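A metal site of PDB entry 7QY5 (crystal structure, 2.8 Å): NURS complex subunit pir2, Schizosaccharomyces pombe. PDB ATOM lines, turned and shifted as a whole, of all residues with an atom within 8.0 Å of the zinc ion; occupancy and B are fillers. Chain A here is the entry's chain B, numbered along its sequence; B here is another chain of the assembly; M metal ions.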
ATOM      1  N   VAL A 263      18.506   5.759  14.068  1.00  0.00           N
ATOM      2  CA  VAL A 263      19.365   5.168  13.004  1.00  0.00           C
ATOM      3  C   VAL A 263      20.376   4.178  13.605  1.00  0.00           C
ATOM      4  O   VAL A 263      21.219   3.686  12.816  1.00  0.00           O
ATOM      5  CB  VAL A 263      20.093   6.268  12.203  1.00  0.00           C
ATOM      6  CG1 VAL A 263      19.125   7.242  11.568  1.00  0.00           C
ATOM      7  CG2 VAL A 263      21.104   7.015  13.055  1.00  0.00           C
ATOM      8  N   ARG A 273      24.051  -1.869  14.982  1.00  0.00           N
ATOM      9  CA  ARG A 273      24.090  -1.584  13.523  1.00  0.00           C
ATOM     10  C   ARG A 273      23.715  -0.119  13.235  1.00  0.00           C
ATOM     11  O   ARG A 273      22.765   0.389  13.858  1.00  0.00           O
ATOM     12  CB  ARG A 273      23.178  -2.514  12.723  1.00  0.00           C
ATOM     13  CG  ARG A 273      23.067  -2.150  11.245  1.00  0.00           C
ATOM     14  CD  ARG A 273      22.835  -3.290  10.266  1.00  0.00           C
ATOM     15  NE  ARG A 273      22.587  -4.567  10.918  1.00  0.00           N
ATOM     16  CZ  ARG A 273      23.526  -5.461  11.222  1.00  0.00           C
ATOM     17  NH1 ARG A 273      24.803  -5.255  10.935  1.00  0.00           N
ATOM     18  NH2 ARG A 273      23.165  -6.580  11.838  1.00  0.00           N
ATOM     19  N   CYS A 274      24.452   0.487  12.296  1.00  0.00           N
ATOM     20  CA  CYS A 274      24.226   1.820  11.658  1.00  0.00           C
ATOM     21  C   CYS A 274      23.288   1.661  10.453  1.00  0.00           C
ATOM     22  O   CYS A 274      23.685   0.962   9.496  1.00  0.00           O
ATOM     23  CB  CYS A 274      25.567   2.392  11.215  1.00  0.00           C
ATOM     24  SG  CYS A 274      25.464   3.773  10.059  1.00  0.00           S
ATOM     25  N   HIS A 275      22.107   2.294  10.504  1.00  0.00           N
ATOM     26  CA  HIS A 275      21.022   2.176   9.485  1.00  0.00           C
ATOM     27  C   HIS A 275      20.948   3.433   8.608  1.00  0.00           C
ATOM     28  O   HIS A 275      19.989   3.553   7.830  1.00  0.00           O
ATOM     29  CB  HIS A 275      19.668   1.851  10.167  1.00  0.00           C
ATOM     30  CG  HIS A 275      19.520   0.414  10.545  1.00  0.00           C
ATOM     31  ND1 HIS A 275      18.868  -0.504   9.740  1.00  0.00           N
ATOM     32  CD2 HIS A 275      19.926  -0.269  11.636  1.00  0.00           C
ATOM     33  CE1 HIS A 275      18.880  -1.691  10.327  1.00  0.00           C
ATOM     34  NE2 HIS A 275      19.521  -1.571  11.489  1.00  0.00           N
ATOM     35  N   VAL A 276      21.964   4.312   8.696  1.00  0.00           N
ATOM     36  CA  VAL A 276      22.097   5.565   7.887  1.00  0.00           C
ATOM     37  C   VAL A 276      22.400   5.188   6.433  1.00  0.00           C
ATOM     38  O   VAL A 276      23.483   4.608   6.197  1.00  0.00           O
ATOM     39  CB  VAL A 276      23.179   6.494   8.473  1.00  0.00           C
ATOM     40  CG1 VAL A 276      23.613   7.581   7.489  1.00  0.00           C
ATOM     41  CG2 VAL A 276      22.707   7.110   9.775  1.00  0.00           C
ATOM     42  N   GLY A 277      21.502   5.541   5.509  1.00  0.00           N
ATOM     43  CA  GLY A 277      21.592   5.211   4.069  1.00  0.00           C
ATOM     44  C   GLY A 277      21.957   3.749   3.861  1.00  0.00           C
ATOM     45  O   GLY A 277      21.580   2.925   4.724  1.00  0.00           O
ATOM     46  N   THR A 278      22.665   3.437   2.770  1.00  0.00           N
ATOM     47  CA  THR A 278      23.146   2.063   2.436  1.00  0.00           C
ATOM     48  C   THR A 278      24.378   1.741   3.293  1.00  0.00           C
ATOM     49  O   THR A 278      25.506   1.728   2.749  1.00  0.00           O
ATOM     50  CB  THR A 278      23.438   1.894   0.930  1.00  0.00           C
ATOM     51  OG1 THR A 278      24.147   3.039   0.467  1.00  0.00           O
ATOM     52  CG2 THR A 278      22.193   1.689   0.106  1.00  0.00           C
ATOM     53  N   CYS A 279      24.153   1.521   4.589  1.00  0.00           N
ATOM     54  CA  CYS A 279      25.175   1.062   5.557  1.00  0.00           C
ATOM     55  C   CYS A 279      24.580  -0.090   6.349  1.00  0.00           C
ATOM     56  O   CYS A 279      23.345  -0.156   6.431  1.00  0.00           O
ATOM     57  CB  CYS A 279      25.617   2.183   6.483  1.00  0.00           C
ATOM     58  SG  CYS A 279      27.298   1.963   7.112  1.00  0.00           S
ATOM     59  N   ALA A 280      25.438  -0.979   6.874  1.00  0.00           N
ATOM     60  CA  ALA A 280      25.055  -2.085   7.773  1.00  0.00           C
ATOM     61  C   ALA A 280      26.217  -2.499   8.679  1.00  0.00           C
ATOM     62  O   ALA A 280      26.191  -3.628   9.187  1.00  0.00           O
ATOM     63  CB  ALA A 280      24.550  -3.254   6.957  1.00  0.00           C
ATOM     64  N   LYS A 281      27.203  -1.612   8.897  1.00  0.00           N
ATOM     65  CA  LYS A 281      28.362  -1.857   9.793  1.00  0.00           C
ATOM     66  C   LYS A 281      27.855  -2.084  11.234  1.00  0.00           C
ATOM     67  O   LYS A 281      26.867  -1.427  11.623  1.00  0.00           O
ATOM     68  CB  LYS A 281      29.351  -0.692   9.737  1.00  0.00           C
ATOM     69  CG  LYS A 281      30.337  -0.700   8.573  1.00  0.00           C
ATOM     70  CD  LYS A 281      31.535   0.204   8.812  1.00  0.00           C
ATOM     71  CE  LYS A 281      32.199   0.686   7.547  1.00  0.00           C
ATOM     72  NZ  LYS A 281      33.530   1.299   7.825  1.00  0.00           N
ATOM     73  N   LEU A 282      28.533  -2.967  11.981  1.00  0.00           N
ATOM     74  CA  LEU A 282      28.149  -3.423  13.353  1.00  0.00           C
ATOM     75  C   LEU A 282      29.230  -3.014  14.353  1.00  0.00           C
ATOM     76  O   LEU A 282      30.422  -3.086  13.992  1.00  0.00           O
ATOM     77  CB  LEU A 282      27.963  -4.940  13.314  1.00  0.00           C
ATOM     78  CG  LEU A 282      27.137  -5.541  14.452  1.00  0.00           C
ATOM     79  CD1 LEU A 282      25.677  -5.139  14.332  1.00  0.00           C
ATOM     80  CD2 LEU A 282      27.275  -7.053  14.466  1.00  0.00           C
ATOM     81  N   PHE A 283      28.858  -2.608  15.579  1.00  0.00           N
ATOM     82  CA  PHE A 283      29.794  -2.089  16.614  1.00  0.00           C
ATOM     83  C   PHE A 283      29.454  -2.666  17.998  1.00  0.00           C
ATOM     84  O   PHE A 283      28.269  -3.037  18.239  1.00  0.00           O
ATOM     85  CB  PHE A 283      29.770  -0.561  16.615  1.00  0.00           C
ATOM     86  CG  PHE A 283      30.203   0.091  15.323  1.00  0.00           C
ATOM     87  CD1 PHE A 283      31.498   0.537  15.144  1.00  0.00           C
ATOM     88  CD2 PHE A 283      29.299   0.254  14.280  1.00  0.00           C
ATOM     89  CE1 PHE A 283      31.898   1.124  13.948  1.00  0.00           C
ATOM     90  CE2 PHE A 283      29.702   0.852  13.092  1.00  0.00           C
ATOM     91  CZ  PHE A 283      30.988   1.282  12.926  1.00  0.00           C
ATOM     92  N   VAL A 289      29.223   3.632  17.109  1.00  0.00           N
ATOM     93  CA  VAL A 289      28.408   3.930  15.895  1.00  0.00           C
ATOM     94  C   VAL A 289      28.340   5.450  15.750  1.00  0.00           C
ATOM     95  O   VAL A 289      28.665   5.937  14.665  1.00  0.00           O
ATOM     96  CB  VAL A 289      26.998   3.322  15.951  1.00  0.00           C
ATOM     97  CG1 VAL A 289      26.314   3.406  14.592  1.00  0.00           C
ATOM     98  CG2 VAL A 289      26.992   1.876  16.444  1.00  0.00           C
ATOM     99  N   HIS A 292      31.342   6.566  14.109  1.00  0.00           N
ATOM    100  CA  HIS A 292      31.259   6.036  12.725  1.00  0.00           C
ATOM    101  C   HIS A 292      30.423   6.990  11.856  1.00  0.00           C
ATOM    102  O   HIS A 292      30.909   7.391  10.774  1.00  0.00           O
ATOM    103  CB  HIS A 292      30.702   4.604  12.742  1.00  0.00           C
ATOM    104  CG  HIS A 292      30.120   4.158  11.446  1.00  0.00           C
ATOM    105  ND1 HIS A 292      30.868   4.061  10.286  1.00  0.00           N
ATOM    106  CD2 HIS A 292      28.862   3.770  11.119  1.00  0.00           C
ATOM    107  CE1 HIS A 292      30.096   3.634   9.302  1.00  0.00           C
ATOM    108  NE2 HIS A 292      28.860   3.449   9.784  1.00  0.00           N
ATOM    109  N   ILE A 293      29.244   7.359  12.373  1.00  0.00           N
ATOM    110  CA  ILE A 293      28.315   8.373  11.803  1.00  0.00           C
ATOM    111  C   ILE A 293      29.109   9.663  11.528  1.00  0.00           C
ATOM    112  O   ILE A 293      29.072  10.125  10.372  1.00  0.00           O
ATOM    113  CB  ILE A 293      27.116   8.616  12.751  1.00  0.00           C
ATOM    114  CG1 ILE A 293      26.271   7.358  13.015  1.00  0.00           C
ATOM    115  CG2 ILE A 293      26.243   9.765  12.256  1.00  0.00           C
ATOM    116  CD1 ILE A 293      25.401   6.944  11.866  1.00  0.00           C
ATOM    117  N   LYS A 296      32.228   8.628   8.775  1.00  0.00           N
ATOM    118  CA  LYS A 296      31.751   8.182   7.446  1.00  0.00           C
ATOM    119  C   LYS A 296      30.589   9.078   6.970  1.00  0.00           C
ATOM    120  O   LYS A 296      30.749   9.705   5.913  1.00  0.00           O
ATOM    121  CB  LYS A 296      31.325   6.706   7.494  1.00  0.00           C
ATOM    122  CG  LYS A 296      30.882   6.108   6.162  1.00  0.00           C
ATOM    123  CD  LYS A 296      30.551   4.644   6.265  1.00  0.00           C
ATOM    124  CE  LYS A 296      30.130   4.009   4.965  1.00  0.00           C
ATOM    125  NZ  LYS A 296      29.845   2.567   5.169  1.00  0.00           N
ATOM    126  N   HIS A 297      29.490   9.145   7.731  1.00  0.00           N
ATOM    127  CA  HIS A 297      28.230   9.824   7.342  1.00  0.00           C
ATOM    128  C   HIS A 297      28.189  11.282   7.832  1.00  0.00           C
ATOM    129  O   HIS A 297      27.103  11.718   8.236  1.00  0.00           O
ATOM    130  CB  HIS A 297      27.024   9.040   7.877  1.00  0.00           C
ATOM    131  CG  HIS A 297      27.063   7.591   7.539  1.00  0.00           C
ATOM    132  ND1 HIS A 297      26.799   7.125   6.271  1.00  0.00           N
ATOM    133  CD2 HIS A 297      27.311   6.507   8.294  1.00  0.00           C
ATOM    134  CE1 HIS A 297      26.885   5.811   6.255  1.00  0.00           C
ATOM    135  NE2 HIS A 297      27.196   5.407   7.499  1.00  0.00           N
ATOM    136  N   GLU B  13      37.340   0.039  11.663  1.00  0.00           N
ATOM    137  CA  GLU B  13      36.916   1.226  12.470  1.00  0.00           C
ATOM    138  C   GLU B  13      37.051   0.902  13.971  1.00  0.00           C
ATOM    139  O   GLU B  13      37.377  -0.250  14.304  1.00  0.00           O
ATOM    140  CB  GLU B  13      35.475   1.647  12.161  1.00  0.00           C
ATOM    141  CG  GLU B  13      35.292   2.329  10.807  1.00  0.00           C
ATOM    142  CD  GLU B  13      34.309   3.493  10.785  1.00  0.00           C
ATOM    143  OE1 GLU B  13      34.183   4.183  11.816  1.00  0.00           O
ATOM    144  OE2 GLU B  13      33.685   3.734   9.723  1.00  0.00           O
HETATM  145 ZN    ZN M   1      26.969   3.506   8.819  1.00  0.00          ZN
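Of the 18 residues printed, 4 come within 4 Å of the zinc ion.
The nearest printed residue that does not touch the zinc ion is Val 276 (4.5 Å).
The backbone NH (N) of Val 276 lies close to the side-chain sulfur (SG) of Cys 274, at 3.8 Å.
The backbone NH of Cys 274 is in hydrogen-bond range of the backbone carbonyl oxygen of Lys 281 (3.2 Å).
A ring nitrogen (ND1) of His 292 sits at hydrogen-bond distance from the side-chain carboxylate (OE2) of Glu 13 of chain B, 2.9 Å away.
SG of Cys 279 sits close to NZ of Lys 296.
The zinc ion is bound by SG of Cys 274, NE2 of His 292, SG of Cys 279 and NE2 of His 297.
The zinc ion has four donor atoms within binding distance.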
